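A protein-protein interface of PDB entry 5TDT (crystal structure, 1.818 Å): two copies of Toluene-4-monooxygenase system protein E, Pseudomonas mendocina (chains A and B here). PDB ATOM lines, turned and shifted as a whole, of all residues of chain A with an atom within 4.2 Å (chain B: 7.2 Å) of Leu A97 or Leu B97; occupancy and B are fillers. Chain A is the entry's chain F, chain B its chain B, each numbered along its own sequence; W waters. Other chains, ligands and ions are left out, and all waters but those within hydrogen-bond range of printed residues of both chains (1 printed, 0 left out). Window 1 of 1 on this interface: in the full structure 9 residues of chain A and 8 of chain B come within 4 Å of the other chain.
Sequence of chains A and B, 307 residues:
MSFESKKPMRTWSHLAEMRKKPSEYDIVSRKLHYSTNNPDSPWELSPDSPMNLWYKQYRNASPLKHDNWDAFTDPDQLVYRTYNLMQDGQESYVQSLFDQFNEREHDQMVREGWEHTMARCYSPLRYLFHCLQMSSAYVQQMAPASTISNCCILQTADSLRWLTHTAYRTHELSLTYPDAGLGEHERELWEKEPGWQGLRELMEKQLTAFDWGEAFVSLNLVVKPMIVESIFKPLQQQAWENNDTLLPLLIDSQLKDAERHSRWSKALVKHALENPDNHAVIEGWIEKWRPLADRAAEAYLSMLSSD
Tyr B93 touches its own counterpart, Tyr A93.
Tyr A93 touches Ser B96, and with the chains exchanged Ser A96 touches Tyr B93.
Leu A97 touches its own counterpart, Leu B97.
Phe A101 touches Leu B249, but with the chains exchanged Leu A249 does not touch Phe B101 (4.05 Å).
Positions printed for both chains: 93, 94, 95, 96, 97, 98, 99, 100, 101 and 249.
Leu A97 touches just these residues of chain B: Tyr B93 (3.9 Å) and Leu B97 (3.9 Å).
Leu B97 touches two residues of chain A.
Printed residues of chain A within 4 Å of Ser B96: Tyr A93 (3.4 Å).
Of the printed residues of chain B, Ser A96 touches Tyr B93 (3.4 Å).
Printed residues of chain A within 4 Å of Leu B249: Phe A101 (3.8 Å).
O of Ser B92 sits at hydrogen-bond distance from OG of Ser B96 (3.0 Å).
Among the printed residues, pairs that only touch across the chains: Tyr A93 with Tyr B93 (3.7 Å), Tyr A93 with Ser B96 (3.4 Å), Tyr A93 with Leu B97 (3.8 Å), Ser A96 with Tyr B93 (3.4 Å), Leu A97 with Tyr B93 (3.9 Å), Leu A97 with Leu B97 (3.9 Å) and Phe A101 with Leu B249 (3.8 Å).
Water W1 bridges OG of Ser A96 (2.9 Å) and NE2 of Gln B90 (3.0 Å).
Printed residues of chain B that touch a printed residue of chain A: Tyr B93, Ser B96, Leu B97 and Leu B249.
Hydrophobic or aromatic side chains of chain B within 4 Å of the printed part of chain A: Tyr B93, Leu B97 and Leu B249.
Printed residues of chain A that touch a printed residue of chain B: Tyr A93, Ser A96, Leu A97 and Phe A101.
Along chain A the printed residues that touch a printed residue of chain B span positions 93 to 101.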
ATOM      1  N   TYR A  93       7.836 -25.141 -36.807  1.00  0.00           N
ATOM      2  CA  TYR A  93       8.040 -25.344 -35.374  1.00  0.00           C
ATOM      3  C   TYR A  93       8.278 -26.822 -35.052  1.00  0.00           C
ATOM      4  O   TYR A  93       9.236 -27.165 -34.351  1.00  0.00           O
ATOM      5  CB  TYR A  93       6.833 -24.791 -34.610  1.00  0.00           C
ATOM      6  CG  TYR A  93       6.627 -25.324 -33.198  1.00  0.00           C
ATOM      7  CD1 TYR A  93       7.469 -24.950 -32.154  1.00  0.00           C
ATOM      8  CD2 TYR A  93       5.564 -26.167 -32.910  1.00  0.00           C
ATOM      9  CE1 TYR A  93       7.262 -25.420 -30.851  1.00  0.00           C
ATOM     10  CE2 TYR A  93       5.343 -26.640 -31.611  1.00  0.00           C
ATOM     11  CZ  TYR A  93       6.194 -26.268 -30.594  1.00  0.00           C
ATOM     12  OH  TYR A  93       5.971 -26.764 -29.332  1.00  0.00           O
ATOM     13  N   VAL A  94       7.424 -27.711 -35.571  1.00  0.00           N
ATOM     14  CA  VAL A  94       7.602 -29.147 -35.330  1.00  0.00           C
ATOM     15  C   VAL A  94       8.943 -29.626 -35.882  1.00  0.00           C
ATOM     16  O   VAL A  94       9.672 -30.370 -35.219  1.00  0.00           O
ATOM     17  CB  VAL A  94       6.435 -29.958 -35.934  1.00  0.00           C
ATOM     18  CG1 VAL A  94       6.789 -31.431 -35.931  1.00  0.00           C
ATOM     19  CG2 VAL A  94       5.152 -29.726 -35.157  1.00  0.00           C
ATOM     20  N   GLN A  95       9.290 -29.210 -37.106  1.00  0.00           N
ATOM     21  CA  GLN A  95      10.581 -29.605 -37.676  1.00  0.00           C
ATOM     22  C   GLN A  95      11.748 -29.036 -36.869  1.00  0.00           C
ATOM     23  O   GLN A  95      12.795 -29.694 -36.732  1.00  0.00           O
ATOM     24  CB  GLN A  95      10.661 -29.172 -39.148  1.00  0.00           C
ATOM     25  CG  GLN A  95       9.518 -29.732 -40.033  1.00  0.00           C
ATOM     26  CD  GLN A  95       9.601 -31.244 -40.208  1.00  0.00           C
ATOM     27  OE1 GLN A  95      10.669 -31.773 -40.520  1.00  0.00           O
ATOM     28  NE2 GLN A  95       8.477 -31.944 -40.007  1.00  0.00           N
ATOM     29  N   SER A  96      11.583 -27.837 -36.305  1.00  0.00           N
ATOM     30  CA  SER A  96      12.620 -27.287 -35.432  1.00  0.00           C
ATOM     31  C   SER A  96      12.732 -28.087 -34.140  1.00  0.00           C
ATOM     32  O   SER A  96      13.843 -28.289 -33.629  1.00  0.00           O
ATOM     33  CB  SER A  96      12.344 -25.814 -35.128  1.00  0.00           C
ATOM     34  OG  SER A  96      12.676 -25.001 -36.239  1.00  0.00           O
ATOM     35  N   LEU A  97      11.598 -28.555 -33.604  1.00  0.00           N
ATOM     36  CA  LEU A  97      11.635 -29.472 -32.467  1.00  0.00           C
ATOM     37  C   LEU A  97      12.391 -30.749 -32.825  1.00  0.00           C
ATOM     38  O   LEU A  97      13.255 -31.198 -32.068  1.00  0.00           O
ATOM     39  CB  LEU A  97      10.216 -29.819 -32.009  1.00  0.00           C
ATOM     40  CG  LEU A  97       9.406 -28.793 -31.222  1.00  0.00           C
ATOM     41  CD1 LEU A  97       7.985 -29.280 -31.069  1.00  0.00           C
ATOM     42  CD2 LEU A  97      10.037 -28.529 -29.857  1.00  0.00           C
ATOM     43  N   PHE A  98      12.062 -31.358 -33.973  1.00  0.00           N
ATOM     44  CA  PHE A  98      12.780 -32.559 -34.408  1.00  0.00           C
ATOM     45  C   PHE A  98      14.283 -32.309 -34.436  1.00  0.00           C
ATOM     46  O   PHE A  98      15.074 -33.110 -33.926  1.00  0.00           O
ATOM     47  CB  PHE A  98      12.310 -33.005 -35.800  1.00  0.00           C
ATOM     48  CG  PHE A  98      10.908 -33.573 -35.841  1.00  0.00           C
ATOM     49  CD1 PHE A  98      10.218 -33.866 -34.680  1.00  0.00           C
ATOM     50  CD2 PHE A  98      10.289 -33.819 -37.067  1.00  0.00           C
ATOM     51  CE1 PHE A  98       8.928 -34.390 -34.729  1.00  0.00           C
ATOM     52  CE2 PHE A  98       8.995 -34.350 -37.123  1.00  0.00           C
ATOM     53  CZ  PHE A  98       8.315 -34.627 -35.960  1.00  0.00           C
ATOM     54  N   ASP A  99      14.691 -31.193 -35.039  1.00  0.00           N
ATOM     55  CA  ASP A  99      16.113 -30.907 -35.193  1.00  0.00           C
ATOM     56  C   ASP A  99      16.813 -30.815 -33.837  1.00  0.00           C
ATOM     57  O   ASP A  99      17.860 -31.445 -33.622  1.00  0.00           O
ATOM     58  CB  ASP A  99      16.287 -29.614 -35.989  1.00  0.00           C
ATOM     59  CG  ASP A  99      17.716 -29.385 -36.454  1.00  0.00           C
ATOM     60  OD1 ASP A  99      18.552 -30.311 -36.377  1.00  0.00           O
ATOM     61  OD2 ASP A  99      17.993 -28.269 -36.929  1.00  0.00           O
ATOM     62  N   GLN A 100      16.234 -30.057 -32.896  1.00  0.00           N
ATOM     63  CA  GLN A 100      16.905 -29.789 -31.622  1.00  0.00           C
ATOM     64  C   GLN A 100      16.893 -31.008 -30.707  1.00  0.00           C
ATOM     65  O   GLN A 100      17.867 -31.259 -29.977  1.00  0.00           O
ATOM     66  CB  GLN A 100      16.253 -28.594 -30.920  1.00  0.00           C
ATOM     67  CG  GLN A 100      16.997 -28.143 -29.654  1.00  0.00           C
ATOM     68  CD  GLN A 100      18.478 -27.877 -29.903  1.00  0.00           C
ATOM     69  OE1 GLN A 100      19.330 -28.280 -29.112  1.00  0.00           O
ATOM     70  NE2 GLN A 100      18.791 -27.196 -31.006  1.00  0.00           N
ATOM     71  N   PHE A 101      15.791 -31.757 -30.703  1.00  0.00           N
ATOM     72  CA  PHE A 101      15.734 -32.938 -29.856  1.00  0.00           C
ATOM     73  C   PHE A 101      16.668 -34.018 -30.380  1.00  0.00           C
ATOM     74  O   PHE A 101      17.253 -34.770 -29.590  1.00  0.00           O
ATOM     75  CB  PHE A 101      14.293 -33.438 -29.749  1.00  0.00           C
ATOM     76  CG  PHE A 101      13.483 -32.719 -28.706  1.00  0.00           C
ATOM     77  CD1 PHE A 101      13.088 -31.403 -28.902  1.00  0.00           C
ATOM     78  CD2 PHE A 101      13.109 -33.359 -27.529  1.00  0.00           C
ATOM     79  CE1 PHE A 101      12.347 -30.732 -27.941  1.00  0.00           C
ATOM     80  CE2 PHE A 101      12.359 -32.701 -26.563  1.00  0.00           C
ATOM     81  CZ  PHE A 101      11.984 -31.382 -26.762  1.00  0.00           C
ATOM     82  N   LEU A 249       4.879 -32.843 -27.120  1.00  0.00           N
ATOM     83  CA  LEU A 249       4.863 -31.599 -27.896  1.00  0.00           C
ATOM     84  C   LEU A 249       4.384 -31.839 -29.327  1.00  0.00           C
ATOM     85  O   LEU A 249       3.638 -31.019 -29.893  1.00  0.00           O
ATOM     86  CB  LEU A 249       6.261 -30.967 -27.896  1.00  0.00           C
ATOM     87  CG  LEU A 249       6.719 -30.445 -26.522  1.00  0.00           C
ATOM     88  CD1 LEU A 249       8.229 -30.180 -26.484  1.00  0.00           C
ATOM     89  CD2 LEU A 249       5.931 -29.195 -26.149  1.00  0.00           C
ATOM     90  N   GLN B  90      13.726 -19.301 -36.647  1.00  0.00           N
ATOM     91  CA  GLN B  90      14.142 -19.613 -35.274  1.00  0.00           C
ATOM     92  C   GLN B  90      13.292 -18.871 -34.253  1.00  0.00           C
ATOM     93  O   GLN B  90      12.912 -19.438 -33.220  1.00  0.00           O
ATOM     94  CB  GLN B  90      15.620 -19.273 -35.054  1.00  0.00           C
ATOM     95  CG  GLN B  90      16.609 -20.154 -35.785  1.00  0.00           C
ATOM     96  CD  GLN B  90      16.262 -21.629 -35.688  1.00  0.00           C
ATOM     97  OE1 GLN B  90      16.300 -22.223 -34.603  1.00  0.00           O
ATOM     98  NE2 GLN B  90      15.900 -22.224 -36.826  1.00  0.00           N
ATOM     99  N   GLU B  91      12.975 -17.603 -34.519  1.00  0.00           N
ATOM    100  CA  GLU B  91      12.223 -16.834 -33.536  1.00  0.00           C
ATOM    101  C   GLU B  91      10.759 -17.265 -33.498  1.00  0.00           C
ATOM    102  O   GLU B  91      10.142 -17.281 -32.427  1.00  0.00           O
ATOM    103  CB  GLU B  91      12.359 -15.334 -33.829  1.00  0.00           C
ATOM    104  CG  GLU B  91      11.858 -14.406 -32.739  1.00  0.00           C
ATOM    105  CD  GLU B  91      12.484 -14.641 -31.356  1.00  0.00           C
ATOM    106  OE1 GLU B  91      13.510 -15.354 -31.243  1.00  0.00           O
ATOM    107  OE2 GLU B  91      11.941 -14.077 -30.375  1.00  0.00           O
ATOM    108  N   SER B  92      10.181 -17.630 -34.644  1.00  0.00           N
ATOM    109  CA  SER B  92       8.818 -18.149 -34.587  1.00  0.00           C
ATOM    110  C   SER B  92       8.789 -19.499 -33.882  1.00  0.00           C
ATOM    111  O   SER B  92       7.789 -19.838 -33.243  1.00  0.00           O
ATOM    112  CB  SER B  92       8.199 -18.242 -35.990  1.00  0.00           C
ATOM    113  OG  SER B  92       8.811 -19.249 -36.765  1.00  0.00           O
ATOM    114  N   TYR B  93       9.889 -20.252 -33.938  1.00  0.00           N
ATOM    115  CA  TYR B  93       9.989 -21.480 -33.150  1.00  0.00           C
ATOM    116  C   TYR B  93      10.002 -21.179 -31.648  1.00  0.00           C
ATOM    117  O   TYR B  93       9.241 -21.791 -30.885  1.00  0.00           O
ATOM    118  CB  TYR B  93      11.228 -22.263 -33.583  1.00  0.00           C
ATOM    119  CG  TYR B  93      11.774 -23.248 -32.577  1.00  0.00           C
ATOM    120  CD1 TYR B  93      11.094 -24.427 -32.259  1.00  0.00           C
ATOM    121  CD2 TYR B  93      12.998 -23.024 -31.988  1.00  0.00           C
ATOM    122  CE1 TYR B  93      11.632 -25.342 -31.354  1.00  0.00           C
ATOM    123  CE2 TYR B  93      13.533 -23.917 -31.091  1.00  0.00           C
ATOM    124  CZ  TYR B  93      12.862 -25.069 -30.772  1.00  0.00           C
ATOM    125  OH  TYR B  93      13.457 -25.921 -29.862  1.00  0.00           O
ATOM    126  N   VAL B  94      10.838 -20.223 -31.209  1.00  0.00           N
ATOM    127  CA  VAL B  94      10.903 -19.854 -29.791  1.00  0.00           C
ATOM    128  C   VAL B  94       9.567 -19.301 -29.303  1.00  0.00           C
ATOM    129  O   VAL B  94       9.105 -19.624 -28.197  1.00  0.00           O
ATOM    130  CB  VAL B  94      12.038 -18.840 -29.539  1.00  0.00           C
ATOM    131  CG1 VAL B  94      11.856 -18.188 -28.152  1.00  0.00           C
ATOM    132  CG2 VAL B  94      13.412 -19.509 -29.665  1.00  0.00           C
ATOM    133  N   GLN B  95       8.933 -18.441 -30.103  1.00  0.00           N
ATOM    134  CA  GLN B  95       7.638 -17.902 -29.703  1.00  0.00           C
ATOM    135  C   GLN B  95       6.573 -18.998 -29.631  1.00  0.00           C
ATOM    136  O   GLN B  95       5.678 -18.939 -28.774  1.00  0.00           O
ATOM    137  CB  GLN B  95       7.223 -16.778 -30.664  1.00  0.00           C
ATOM    138  CG  GLN B  95       8.208 -15.575 -30.692  1.00  0.00           C
ATOM    139  CD  GLN B  95       8.251 -14.799 -29.377  1.00  0.00           C
ATOM    140  OE1 GLN B  95       7.214 -14.496 -28.804  1.00  0.00           O
ATOM    141  NE2 GLN B  95       9.450 -14.469 -28.907  1.00  0.00           N
ATOM    142  N   SER B  96       6.654 -20.011 -30.500  1.00  0.00           N
ATOM    143  CA  SER B  96       5.745 -21.150 -30.382  1.00  0.00           C
ATOM    144  C   SER B  96       6.009 -21.947 -29.106  1.00  0.00           C
ATOM    145  O   SER B  96       5.064 -22.439 -28.480  1.00  0.00           O
ATOM    146  CB  SER B  96       5.851 -22.050 -31.612  1.00  0.00           C
ATOM    147  OG  SER B  96       5.261 -21.434 -32.752  1.00  0.00           O
ATOM    148  N   LEU B  97       7.282 -22.091 -28.704  1.00  0.00           N
ATOM    149  CA  LEU B  97       7.597 -22.719 -27.417  1.00  0.00           C
ATOM    150  C   LEU B  97       6.984 -21.935 -26.261  1.00  0.00           C
ATOM    151  O   LEU B  97       6.371 -22.519 -25.355  1.00  0.00           O
ATOM    152  CB  LEU B  97       9.114 -22.832 -27.213  1.00  0.00           C
ATOM    153  CG  LEU B  97       9.914 -23.843 -28.023  1.00  0.00           C
ATOM    154  CD1 LEU B  97      11.413 -23.687 -27.743  1.00  0.00           C
ATOM    155  CD2 LEU B  97       9.464 -25.262 -27.726  1.00  0.00           C
ATOM    156  N   PHE B  98       7.161 -20.609 -26.261  1.00  0.00           N
ATOM    157  CA  PHE B  98       6.570 -19.788 -25.210  1.00  0.00           C
ATOM    158  C   PHE B  98       5.075 -20.054 -25.118  1.00  0.00           C
ATOM    159  O   PHE B  98       4.555 -20.365 -24.044  1.00  0.00           O
ATOM    160  CB  PHE B  98       6.816 -18.294 -25.463  1.00  0.00           C
ATOM    161  CG  PHE B  98       8.248 -17.846 -25.291  1.00  0.00           C
ATOM    162  CD1 PHE B  98       9.210 -18.668 -24.709  1.00  0.00           C
ATOM    163  CD2 PHE B  98       8.620 -16.573 -25.704  1.00  0.00           C
ATOM    164  CE1 PHE B  98      10.519 -18.227 -24.563  1.00  0.00           C
ATOM    165  CE2 PHE B  98       9.922 -16.127 -25.559  1.00  0.00           C
ATOM    166  CZ  PHE B  98      10.874 -16.962 -24.993  1.00  0.00           C
ATOM    167  N   ASP B  99       4.376 -19.958 -26.255  1.00  0.00           N
ATOM    168  CA  ASP B  99       2.931 -20.197 -26.315  1.00  0.00           C
ATOM    169  C   ASP B  99       2.550 -21.556 -25.718  1.00  0.00           C
ATOM    170  O   ASP B  99       1.709 -21.633 -24.815  1.00  0.00           O
ATOM    171  CB  ASP B  99       2.480 -20.090 -27.773  1.00  0.00           C
ATOM    172  CG  ASP B  99       0.954 -20.066 -27.942  1.00  0.00           C
ATOM    173  OD1 ASP B  99       0.209 -19.838 -26.965  1.00  0.00           O
ATOM    174  OD2 ASP B  99       0.505 -20.270 -29.089  1.00  0.00           O
ATOM    175  N   GLN B 100       3.184 -22.639 -26.194  1.00  0.00           N
ATOM    176  CA  GLN B 100       2.777 -23.981 -25.771  1.00  0.00           C
ATOM    177  C   GLN B 100       3.144 -24.256 -24.316  1.00  0.00           C
ATOM    178  O   GLN B 100       2.353 -24.871 -23.585  1.00  0.00           O
ATOM    179  CB  GLN B 100       3.406 -25.050 -26.674  1.00  0.00           C
ATOM    180  CG  GLN B 100       2.947 -26.503 -26.358  1.00  0.00           C
ATOM    181  CD  GLN B 100       1.426 -26.668 -26.423  1.00  0.00           C
ATOM    182  OE1 GLN B 100       0.777 -26.156 -27.333  1.00  0.00           O
ATOM    183  NE2 GLN B 100       0.852 -27.371 -25.442  1.00  0.00           N
ATOM    184  N   PHE B 101       4.351 -23.857 -23.881  1.00  0.00           N
ATOM    185  CA  PHE B 101       4.716 -24.088 -22.483  1.00  0.00           C
ATOM    186  C   PHE B 101       3.827 -23.278 -21.548  1.00  0.00           C
ATOM    187  O   PHE B 101       3.525 -23.720 -20.434  1.00  0.00           O
ATOM    188  CB  PHE B 101       6.198 -23.762 -22.250  1.00  0.00           C
ATOM    189  CG  PHE B 101       7.117 -24.889 -22.618  1.00  0.00           C
ATOM    190  CD1 PHE B 101       7.263 -25.277 -23.945  1.00  0.00           C
ATOM    191  CD2 PHE B 101       7.811 -25.586 -21.632  1.00  0.00           C
ATOM    192  CE1 PHE B 101       8.103 -26.332 -24.286  1.00  0.00           C
ATOM    193  CE2 PHE B 101       8.658 -26.630 -21.968  1.00  0.00           C
ATOM    194  CZ  PHE B 101       8.799 -27.005 -23.301  1.00  0.00           C
ATOM    195  N   ASN B 102       3.372 -22.108 -21.996  1.00  0.00           N
ATOM    196  CA  ASN B 102       2.432 -21.331 -21.192  1.00  0.00           C
ATOM    197  C   ASN B 102       1.080 -22.035 -21.088  1.00  0.00           C
ATOM    198  O   ASN B 102       0.455 -22.020 -20.020  1.00  0.00           O
ATOM    199  CB  ASN B 102       2.258 -19.932 -21.780  1.00  0.00           C
ATOM    200  CG  ASN B 102       1.092 -19.191 -21.164  1.00  0.00           C
ATOM    201  OD1 ASN B 102      -0.049 -19.367 -21.574  1.00  0.00           O
ATOM    202  ND2 ASN B 102       1.374 -18.367 -20.164  1.00  0.00           N
ATOM    203  N   GLU B 103       0.602 -22.631 -22.190  1.00  0.00           N
ATOM    204  CA  GLU B 103      -0.633 -23.414 -22.143  1.00  0.00           C
ATOM    205  C   GLU B 103      -0.547 -24.495 -21.075  1.00  0.00           C
ATOM    206  O   GLU B 103      -1.517 -24.754 -20.352  1.00  0.00           O
ATOM    207  CB  GLU B 103      -0.915 -24.066 -23.504  1.00  0.00           C
ATOM    208  CG  GLU B 103      -1.353 -23.123 -24.608  1.00  0.00           C
ATOM    209  CD  GLU B 103      -2.696 -22.468 -24.320  1.00  0.00           C
ATOM    210  OE1 GLU B 103      -2.705 -21.239 -24.097  1.00  0.00           O
ATOM    211  OE2 GLU B 103      -3.733 -23.180 -24.311  1.00  0.00           O
ATOM    212  N   GLU B 172       6.677 -12.743 -17.911  1.00  0.00           N
ATOM    213  CA  GLU B 172       5.851 -13.942 -17.858  1.00  0.00           C
ATOM    214  C   GLU B 172       6.013 -14.657 -16.524  1.00  0.00           C
ATOM    215  O   GLU B 172       5.020 -15.026 -15.887  1.00  0.00           O
ATOM    216  CB  GLU B 172       6.187 -14.886 -19.015  1.00  0.00           C
ATOM    217  CG  GLU B 172       5.345 -16.169 -19.000  1.00  0.00           C
ATOM    218  CD  GLU B 172       5.286 -16.859 -20.348  1.00  0.00           C
ATOM    219  OE1 GLU B 172       4.166 -17.132 -20.847  1.00  0.00           O
ATOM    220  OE2 GLU B 172       6.364 -17.120 -20.915  1.00  0.00           O
ATOM    221  N   THR B 245      12.050 -26.892 -17.954  1.00  0.00           N
ATOM    222  CA  THR B 245      12.361 -27.489 -19.252  1.00  0.00           C
ATOM    223  C   THR B 245      12.278 -26.491 -20.405  1.00  0.00           C
ATOM    224  O   THR B 245      12.719 -26.812 -21.516  1.00  0.00           O
ATOM    225  CB  THR B 245      11.446 -28.691 -19.545  1.00  0.00           C
ATOM    226  OG1 THR B 245      10.071 -28.303 -19.455  1.00  0.00           O
ATOM    227  CG2 THR B 245      11.723 -29.823 -18.560  1.00  0.00           C
ATOM    228  N   LEU B 246      11.751 -25.293 -20.164  1.00  0.00           N
ATOM    229  CA  LEU B 246      11.725 -24.258 -21.192  1.00  0.00           C
ATOM    230  C   LEU B 246      13.096 -23.599 -21.346  1.00  0.00           C
ATOM    231  O   LEU B 246      13.581 -23.416 -22.468  1.00  0.00           O
ATOM    232  CB  LEU B 246      10.667 -23.211 -20.838  1.00  0.00           C
ATOM    233  CG  LEU B 246      10.554 -21.939 -21.696  1.00  0.00           C
ATOM    234  CD1 LEU B 246      10.570 -22.276 -23.186  1.00  0.00           C
ATOM    235  CD2 LEU B 246       9.297 -21.130 -21.335  1.00  0.00           C
ATOM    236  N   LEU B 249      15.745 -25.158 -23.693  1.00  0.00           N
ATOM    237  CA  LEU B 249      15.415 -25.019 -25.107  1.00  0.00           C
ATOM    238  C   LEU B 249      15.614 -23.581 -25.580  1.00  0.00           C
ATOM    239  O   LEU B 249      16.062 -23.350 -26.713  1.00  0.00           O
ATOM    240  CB  LEU B 249      13.977 -25.477 -25.364  1.00  0.00           C
ATOM    241  CG  LEU B 249      13.649 -26.981 -25.244  1.00  0.00           C
ATOM    242  CD1 LEU B 249      12.125 -27.229 -25.221  1.00  0.00           C
ATOM    243  CD2 LEU B 249      14.273 -27.812 -26.372  1.00  0.00           C
ATOM    244  N   LEU B 250      15.265 -22.602 -24.742  1.00  0.00           N
ATOM    245  CA  LEU B 250      15.482 -21.208 -25.116  1.00  0.00           C
ATOM    246  C   LEU B 250      16.971 -20.943 -25.297  1.00  0.00           C
ATOM    247  O   LEU B 250      17.399 -20.370 -26.304  1.00  0.00           O
ATOM    248  CB  LEU B 250      14.916 -20.283 -24.042  1.00  0.00           C
ATOM    249  CG  LEU B 250      15.154 -18.767 -24.195  1.00  0.00           C
ATOM    250  CD1 LEU B 250      14.556 -18.244 -25.539  1.00  0.00           C
ATOM    251  CD2 LEU B 250      14.615 -18.009 -22.997  1.00  0.00           C
ATOM    252  N   SER B 253      18.531 -22.113 -28.435  1.00  0.00           N
ATOM    253  CA  SER B 253      18.338 -21.204 -29.565  1.00  0.00           C
ATOM    254  C   SER B 253      19.291 -20.014 -29.498  1.00  0.00           C
ATOM    255  O   SER B 253      19.861 -19.615 -30.520  1.00  0.00           O
ATOM    256  CB  SER B 253      16.889 -20.718 -29.624  1.00  0.00           C
ATOM    257  OG  SER B 253      16.656 -19.959 -30.807  1.00  0.00           O
HETATM  258  O   HOH W   1      15.543 -25.126 -35.980  1.00  0.00           O
